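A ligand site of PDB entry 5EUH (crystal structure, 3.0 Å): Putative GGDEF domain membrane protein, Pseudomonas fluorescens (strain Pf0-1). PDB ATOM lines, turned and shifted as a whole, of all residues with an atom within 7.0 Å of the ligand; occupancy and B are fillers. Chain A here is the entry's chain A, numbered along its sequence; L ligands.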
ATOM      1  N   THR A  67     -15.728 -15.194  31.093  1.00  0.00           N
ATOM      2  CA  THR A  67     -16.416 -16.233  30.328  1.00  0.00           C
ATOM      3  C   THR A  67     -16.914 -15.719  28.987  1.00  0.00           C
ATOM      4  O   THR A  67     -17.110 -16.514  28.068  1.00  0.00           O
ATOM      5  CB  THR A  67     -17.589 -16.799  31.127  1.00  0.00           C
ATOM      6  OG1 THR A  67     -18.505 -15.752  31.442  1.00  0.00           O
ATOM      7  CG2 THR A  67     -17.081 -17.424  32.422  1.00  0.00           C
ATOM      8  N   THR A  68     -17.128 -14.407  28.849  1.00  0.00           N
ATOM      9  CA  THR A  68     -17.461 -13.829  27.556  1.00  0.00           C
ATOM     10  C   THR A  68     -16.265 -13.794  26.622  1.00  0.00           C
ATOM     11  O   THR A  68     -16.432 -13.781  25.397  1.00  0.00           O
ATOM     12  CB  THR A  68     -18.042 -12.426  27.746  1.00  0.00           C
ATOM     13  OG1 THR A  68     -19.187 -12.501  28.611  1.00  0.00           O
ATOM     14  CG2 THR A  68     -18.469 -11.806  26.421  1.00  0.00           C
ATOM     15  N   ASN A  69     -15.051 -13.797  27.163  1.00  0.00           N
ATOM     16  CA  ASN A  69     -13.841 -13.775  26.364  1.00  0.00           C
ATOM     17  C   ASN A  69     -13.136 -15.116  26.319  1.00  0.00           C
ATOM     18  O   ASN A  69     -12.109 -15.239  25.641  1.00  0.00           O
ATOM     19  CB  ASN A  69     -12.885 -12.711  26.882  1.00  0.00           C
ATOM     20  CG  ASN A  69     -13.411 -11.308  26.671  1.00  0.00           C
ATOM     21  OD1 ASN A  69     -13.163 -10.697  25.652  1.00  0.00           O
ATOM     22  ND2 ASN A  69     -14.163 -10.803  27.640  1.00  0.00           N
ATOM     23  N   VAL A  70     -13.650 -16.122  27.012  1.00  0.00           N
ATOM     24  CA  VAL A  70     -13.062 -17.457  27.063  1.00  0.00           C
ATOM     25  C   VAL A  70     -14.171 -18.445  26.735  1.00  0.00           C
ATOM     26  O   VAL A  70     -15.057 -18.674  27.568  1.00  0.00           O
ATOM     27  CB  VAL A  70     -12.440 -17.750  28.442  1.00  0.00           C
ATOM     28  CG1 VAL A  70     -12.079 -19.206  28.569  1.00  0.00           C
ATOM     29  CG2 VAL A  70     -11.215 -16.880  28.646  1.00  0.00           C
ATOM     30  N   ARG A  71     -14.133 -19.018  25.536  1.00  0.00           N
ATOM     31  CA  ARG A  71     -15.308 -19.676  24.992  1.00  0.00           C
ATOM     32  C   ARG A  71     -15.059 -21.032  24.333  1.00  0.00           C
ATOM     33  O   ARG A  71     -16.031 -21.666  23.915  1.00  0.00           O
ATOM     34  CB  ARG A  71     -15.976 -18.753  23.959  1.00  0.00           C
ATOM     35  CG  ARG A  71     -16.458 -17.432  24.525  1.00  0.00           C
ATOM     36  CD  ARG A  71     -16.415 -16.343  23.488  1.00  0.00           C
ATOM     37  NE  ARG A  71     -15.052 -16.068  23.042  1.00  0.00           N
ATOM     38  CZ  ARG A  71     -14.690 -14.932  22.457  1.00  0.00           C
ATOM     39  NH1 ARG A  71     -15.580 -13.976  22.256  1.00  0.00           N
ATOM     40  NH2 ARG A  71     -13.428 -14.751  22.083  1.00  0.00           N
ATOM     41  N   ARG A  72     -13.836 -21.508  24.249  1.00  0.00           N
ATOM     42  CA  ARG A  72     -13.573 -22.722  23.489  1.00  0.00           C
ATOM     43  C   ARG A  72     -13.674 -23.958  24.380  1.00  0.00           C
ATOM     44  O   ARG A  72     -13.625 -23.847  25.612  1.00  0.00           O
ATOM     45  CB  ARG A  72     -12.196 -22.631  22.837  1.00  0.00           C
ATOM     46  CG  ARG A  72     -12.104 -21.528  21.806  1.00  0.00           C
ATOM     47  CD  ARG A  72     -10.750 -21.464  21.136  1.00  0.00           C
ATOM     48  NE  ARG A  72     -10.682 -20.344  20.198  1.00  0.00           N
ATOM     49  CZ  ARG A  72      -9.597 -20.009  19.505  1.00  0.00           C
ATOM     50  NH1 ARG A  72      -8.486 -20.719  19.627  1.00  0.00           N
ATOM     51  NH2 ARG A  72      -9.639 -18.970  18.673  1.00  0.00           N
ATOM     52  N   PRO A  73     -13.854 -25.140  23.783  1.00  0.00           N
ATOM     53  CA  PRO A  73     -14.079 -26.348  24.611  1.00  0.00           C
ATOM     54  C   PRO A  73     -12.950 -26.670  25.565  1.00  0.00           C
ATOM     55  O   PRO A  73     -13.207 -27.103  26.703  1.00  0.00           O
ATOM     56  CB  PRO A  73     -14.258 -27.454  23.566  1.00  0.00           C
ATOM     57  CG  PRO A  73     -14.724 -26.746  22.356  1.00  0.00           C
ATOM     58  CD  PRO A  73     -14.028 -25.423  22.350  1.00  0.00           C
ATOM     59  N   ALA A  74     -11.700 -26.493  25.147  1.00  0.00           N
ATOM     60  CA  ALA A  74     -10.541 -26.848  25.957  1.00  0.00           C
ATOM     61  C   ALA A  74     -10.160 -25.757  26.946  1.00  0.00           C
ATOM     62  O   ALA A  74      -9.081 -25.809  27.534  1.00  0.00           O
ATOM     63  CB  ALA A  74      -9.359 -27.176  25.058  1.00  0.00           C
ATOM     64  N   ASP A  75     -11.027 -24.764  27.147  1.00  0.00           N
ATOM     65  CA  ASP A  75     -10.788 -23.689  28.098  1.00  0.00           C
ATOM     66  C   ASP A  75     -11.616 -23.928  29.358  1.00  0.00           C
ATOM     67  O   ASP A  75     -12.715 -24.473  29.302  1.00  0.00           O
ATOM     68  CB  ASP A  75     -11.142 -22.336  27.499  1.00  0.00           C
ATOM     69  CG  ASP A  75     -10.442 -22.074  26.188  1.00  0.00           C
ATOM     70  OD1 ASP A  75      -9.525 -22.850  25.839  1.00  0.00           O
ATOM     71  OD2 ASP A  75     -10.798 -21.093  25.513  1.00  0.00           O
ATOM     72  N   ILE A  88      -7.759 -21.679  32.213  1.00  0.00           N
ATOM     73  CA  ILE A  88      -6.897 -22.530  31.405  1.00  0.00           C
ATOM     74  C   ILE A  88      -7.175 -22.219  29.936  1.00  0.00           C
ATOM     75  O   ILE A  88      -8.339 -22.164  29.519  1.00  0.00           O
ATOM     76  CB  ILE A  88      -7.136 -24.019  31.702  1.00  0.00           C
ATOM     77  CG1 ILE A  88      -6.951 -24.319  33.183  1.00  0.00           C
ATOM     78  CG2 ILE A  88      -6.198 -24.880  30.878  1.00  0.00           C
ATOM     79  CD1 ILE A  88      -7.212 -25.768  33.536  1.00  0.00           C
ATOM     80  N   LEU A  89      -6.124 -22.011  29.168  1.00  0.00           N
ATOM     81  CA  LEU A  89      -6.208 -21.744  27.741  1.00  0.00           C
ATOM     82  C   LEU A  89      -5.410 -22.830  27.038  1.00  0.00           C
ATOM     83  O   LEU A  89      -4.263 -22.611  26.640  1.00  0.00           O
ATOM     84  CB  LEU A  89      -5.704 -20.360  27.400  1.00  0.00           C
ATOM     85  CG  LEU A  89      -6.399 -19.187  28.084  1.00  0.00           C
ATOM     86  CD1 LEU A  89      -5.678 -17.886  27.745  1.00  0.00           C
ATOM     87  CD2 LEU A  89      -7.851 -19.109  27.664  1.00  0.00           C
ATOM     88  N   ALA A  90      -6.014 -23.996  26.889  1.00  0.00           N
ATOM     89  CA  ALA A  90      -5.345 -25.091  26.209  1.00  0.00           C
ATOM     90  C   ALA A  90      -5.208 -24.785  24.729  1.00  0.00           C
ATOM     91  O   ALA A  90      -6.071 -24.144  24.127  1.00  0.00           O
ATOM     92  CB  ALA A  90      -6.105 -26.397  26.405  1.00  0.00           C
ATOM     93  N   GLU A  91      -4.105 -25.251  24.140  1.00  0.00           N
ATOM     94  CA  GLU A  91      -3.827 -25.072  22.717  1.00  0.00           C
ATOM     95  C   GLU A  91      -3.872 -23.602  22.323  1.00  0.00           C
ATOM     96  O   GLU A  91      -4.338 -23.239  21.237  1.00  0.00           O
ATOM     97  CB  GLU A  91      -4.769 -25.911  21.860  1.00  0.00           C
ATOM     98  CG  GLU A  91      -4.825 -27.356  22.300  1.00  0.00           C
ATOM     99  CD  GLU A  91      -5.615 -28.226  21.365  1.00  0.00           C
ATOM    100  OE1 GLU A  91      -6.128 -27.698  20.357  1.00  0.00           O
ATOM    101  OE2 GLU A  91      -5.712 -29.442  21.623  1.00  0.00           O
ATOM    102  N   THR A  92      -3.386 -22.740  23.215  1.00  0.00           N
ATOM    103  CA  THR A  92      -3.315 -21.304  22.990  1.00  0.00           C
ATOM    104  C   THR A  92      -1.899 -20.840  23.298  1.00  0.00           C
ATOM    105  O   THR A  92      -1.372 -21.120  24.380  1.00  0.00           O
ATOM    106  CB  THR A  92      -4.316 -20.547  23.874  1.00  0.00           C
ATOM    107  OG1 THR A  92      -5.646 -21.010  23.587  1.00  0.00           O
ATOM    108  CG2 THR A  92      -4.239 -19.051  23.618  1.00  0.00           C
ATOM    109  N   ASP A  93      -1.283 -20.134  22.354  1.00  0.00           N
ATOM    110  CA  ASP A  93       0.077 -19.661  22.543  1.00  0.00           C
ATOM    111  C   ASP A  93       0.082 -18.373  23.358  1.00  0.00           C
ATOM    112  O   ASP A  93      -0.966 -17.826  23.712  1.00  0.00           O
ATOM    113  CB  ASP A  93       0.777 -19.477  21.195  1.00  0.00           C
ATOM    114  CG  ASP A  93       0.190 -18.334  20.391  1.00  0.00           C
ATOM    115  OD1 ASP A  93      -0.956 -17.926  20.658  1.00  0.00           O
ATOM    116  OD2 ASP A  93       0.885 -17.851  19.461  1.00  0.00           O
ATOM    117  N   VAL A  95       0.974 -15.320  22.544  1.00  0.00           N
ATOM    118  CA  VAL A  95       0.472 -14.142  21.845  1.00  0.00           C
ATOM    119  C   VAL A  95      -1.051 -14.057  21.951  1.00  0.00           C
ATOM    120  O   VAL A  95      -1.608 -13.004  22.265  1.00  0.00           O
ATOM    121  CB  VAL A  95       0.930 -14.155  20.372  1.00  0.00           C
ATOM    122  CG1 VAL A  95       0.486 -12.887  19.663  1.00  0.00           C
ATOM    123  CG2 VAL A  95       2.439 -14.320  20.295  1.00  0.00           C
ATOM    124  N   GLY A  96      -1.732 -15.175  21.674  1.00  0.00           N
ATOM    125  CA  GLY A  96      -3.175 -15.194  21.768  1.00  0.00           C
ATOM    126  C   GLY A  96      -3.682 -15.042  23.181  1.00  0.00           C
ATOM    127  O   GLY A  96      -4.756 -14.464  23.410  1.00  0.00           O
ATOM    128  N   ALA A  97      -2.929 -15.551  24.167  1.00  0.00           N
ATOM    129  CA  ALA A  97      -3.327 -15.416  25.556  1.00  0.00           C
ATOM    130  C   ALA A  97      -3.300 -13.959  25.998  1.00  0.00           C
ATOM    131  O   ALA A  97      -4.115 -13.541  26.826  1.00  0.00           O
ATOM    132  CB  ALA A  97      -2.427 -16.255  26.454  1.00  0.00           C
ATOM    133  N   GLN A  99      -3.938 -11.341  24.047  1.00  0.00           N
ATOM    134  CA  GLN A  99      -5.099 -10.679  23.461  1.00  0.00           C
ATOM    135  C   GLN A  99      -6.359 -10.944  24.271  1.00  0.00           C
ATOM    136  O   GLN A  99      -7.189 -10.049  24.440  1.00  0.00           O
ATOM    137  CB  GLN A  99      -5.298 -11.155  22.019  1.00  0.00           C
ATOM    138  CG  GLN A  99      -4.045 -11.105  21.166  1.00  0.00           C
ATOM    139  CD  GLN A  99      -4.328 -11.385  19.713  1.00  0.00           C
ATOM    140  OE1 GLN A  99      -4.911 -10.563  19.012  1.00  0.00           O
ATOM    141  NE2 GLN A  99      -3.920 -12.563  19.246  1.00  0.00           N
ATOM    142  N   ILE A 100      -6.515 -12.167  24.768  1.00  0.00           N
ATOM    143  CA  ILE A 100      -7.637 -12.476  25.648  1.00  0.00           C
ATOM    144  C   ILE A 100      -7.554 -11.641  26.915  1.00  0.00           C
ATOM    145  O   ILE A 100      -8.564 -11.111  27.401  1.00  0.00           O
ATOM    146  CB  ILE A 100      -7.656 -13.978  25.992  1.00  0.00           C
ATOM    147  CG1 ILE A 100      -7.720 -14.825  24.719  1.00  0.00           C
ATOM    148  CG2 ILE A 100      -8.823 -14.295  26.918  1.00  0.00           C
ATOM    149  CD1 ILE A 100      -7.440 -16.285  24.975  1.00  0.00           C
ATOM    150  N   HIS A 103      -8.496  -7.962  26.294  1.00  0.00           N
ATOM    151  CA  HIS A 103      -9.938  -7.843  26.179  1.00  0.00           C
ATOM    152  C   HIS A 103     -10.603  -7.879  27.546  1.00  0.00           C
ATOM    153  O   HIS A 103     -11.523  -7.097  27.825  1.00  0.00           O
ATOM    154  CB  HIS A 103     -10.485  -8.962  25.289  1.00  0.00           C
ATOM    155  CG  HIS A 103     -10.221  -8.778  23.831  1.00  0.00           C
ATOM    156  ND1 HIS A 103      -9.989  -7.543  23.262  1.00  0.00           N
ATOM    157  CD2 HIS A 103     -10.154  -9.671  22.815  1.00  0.00           C
ATOM    158  CE1 HIS A 103      -9.794  -7.686  21.967  1.00  0.00           C
ATOM    159  NE2 HIS A 103      -9.880  -8.967  21.666  1.00  0.00           N
HETATM  160  P1  LIG L   1      -6.770 -17.268  16.342  1.00  0.00           P
HETATM  161  O1  LIG L   1      -5.776 -17.224  15.209  1.00  0.00           O
HETATM  162  O2  LIG L   1      -7.235 -18.601  16.891  1.00  0.00           O
HETATM  163  O3  LIG L   1      -8.064 -16.408  15.959  1.00  0.00           O
HETATM  164  C1  LIG L   1      -8.162 -15.817  14.657  1.00  0.00           C
HETATM  165  C2  LIG L   1      -9.480 -15.076  14.483  1.00  0.00           C
HETATM  166  O4  LIG L   1     -10.418 -15.949  13.853  1.00  0.00           O
HETATM  167  C3  LIG L   1     -10.121 -14.618  15.782  1.00  0.00           C
HETATM  168  O5  LIG L   1      -9.838 -13.258  16.069  1.00  0.00           O
HETATM  169  C4  LIG L   1     -11.603 -14.745  15.514  1.00  0.00           C
HETATM  170  O6  LIG L   1     -12.140 -13.492  15.101  1.00  0.00           O
HETATM  171  C5  LIG L   1     -11.725 -15.743  14.387  1.00  0.00           C
HETATM  172  N1  LIG L   1     -12.203 -17.003  14.974  1.00  0.00           N
HETATM  173  C6  LIG L   1     -11.441 -18.086  15.242  1.00  0.00           C
HETATM  174  N2  LIG L   1     -12.190 -19.076  15.789  1.00  0.00           N
HETATM  175  C7  LIG L   1     -13.456 -18.627  15.881  1.00  0.00           C
HETATM  176  C8  LIG L   1     -14.744 -19.151  16.363  1.00  0.00           C
HETATM  177  O7  LIG L   1     -14.821 -20.305  16.833  1.00  0.00           O
HETATM  178  N3  LIG L   1     -15.818 -18.363  16.274  1.00  0.00           N
HETATM  179  C9  LIG L   1     -15.767 -17.122  15.772  1.00  0.00           C
HETATM  180  N4  LIG L   1     -16.910 -16.380  15.729  1.00  0.00           N
HETATM  181  N5  LIG L   1     -14.622 -16.568  15.316  1.00  0.00           N
HETATM  182  C10 LIG L   1     -13.455 -17.259  15.338  1.00  0.00           C
HETATM  183  P2  LIG L   1      -9.706 -12.772  17.603  1.00  0.00           P
HETATM  184  O8  LIG L   1      -9.015 -11.431  17.619  1.00  0.00           O
HETATM  185  O9  LIG L   1     -11.033 -12.932  18.295  1.00  0.00           O
HETATM  186  O10 LIG L   1      -8.701 -13.876  18.193  1.00  0.00           O
HETATM  187  C11 LIG L   1      -7.365 -13.515  18.538  1.00  0.00           C
HETATM  188  C12 LIG L   1      -6.690 -14.698  19.223  1.00  0.00           C
HETATM  189  O11 LIG L   1      -7.157 -14.775  20.556  1.00  0.00           O
HETATM  190  C13 LIG L   1      -7.051 -16.038  18.607  1.00  0.00           C
HETATM  191  O12 LIG L   1      -6.159 -16.426  17.571  1.00  0.00           O
HETATM  192  C14 LIG L   1      -6.971 -17.002  19.765  1.00  0.00           C
HETATM  193  O13 LIG L   1      -5.652 -17.535  19.866  1.00  0.00           O
HETATM  194  C15 LIG L   1      -7.247 -16.130  20.970  1.00  0.00           C
HETATM  195  N6  LIG L   1      -8.629 -16.362  21.442  1.00  0.00           N
HETATM  196  C16 LIG L   1      -9.676 -15.557  21.202  1.00  0.00           C
HETATM  197  N7  LIG L   1     -10.801 -16.040  21.771  1.00  0.00           N
HETATM  198  C17 LIG L   1     -10.469 -17.192  22.382  1.00  0.00           C
HETATM  199  C18 LIG L   1     -11.168 -18.215  23.180  1.00  0.00           C
HETATM  200  O14 LIG L   1     -12.392 -18.116  23.416  1.00  0.00           O
HETATM  201  N8  LIG L   1     -10.460 -19.246  23.639  1.00  0.00           N
HETATM  202  C19 LIG L   1      -9.144 -19.391  23.401  1.00  0.00           C
HETATM  203  N9  LIG L   1      -8.490 -20.473  23.894  1.00  0.00           N
HETATM  204  N10 LIG L   1      -8.431 -18.490  22.681  1.00  0.00           N
HETATM  205  C20 LIG L   1      -9.040 -17.399  22.159  1.00  0.00           C
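OD2 of Asp 75 lies within hydrogen-bond range of N8 of the ligand (2.7 Å). The backbone NH (N) of Arg 71 lies within hydrogen-bond range of an oxygen (O14) of the ligand, 2.9 Å away. NH2 of Arg 71 is in hydrogen-bond range of N7 of the ligand (2.9 Å). A nitrogen (N9) of the ligand lies within hydrogen-bond range of the side-chain hydroxyl (OG1) of Thr 92. NH2 of Arg 72 lies within salt-bridge range of O2 of the ligand, at 3.0 Å.
The backbone NH (N) of Arg 72 lies within hydrogen-bond range of the side-chain carboxylate (OD2) of Asp 75, 3.3 Å away. The guanidinium group (NH1) of Arg 71 sits close to the backbone carbonyl oxygen (O) of Thr 68 (3.3 Å). O of Ala 90 is in hydrogen-bond range of OG1 of Thr 92. The backbone NH of Gly 96 lies within hydrogen-bond range of the side-chain carboxylate of Asp 93 (3.0 Å).
O of Asn 69 touches O14 of the ligand (3.6 Å). Val 70 touches the ligand (CA to O14, 3.8 Å). Gly 96 touches the ligand. Gln 99 touches the ligand. CD1 of Ile 100 touches N10 of the ligand, 3.3 Å away. Hydrophobic or aromatic side chains that line the ligand: Ile 100. Nine residues have an atom within 4 Å of the ligand: Asn 69, Val 70, Arg 71, Arg 72, Asp 75, Thr 92, Gly 96, Gln 99 and Ile 100. The nearest printed residue that does not touch the ligand is Leu 89 (4.1 Å).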
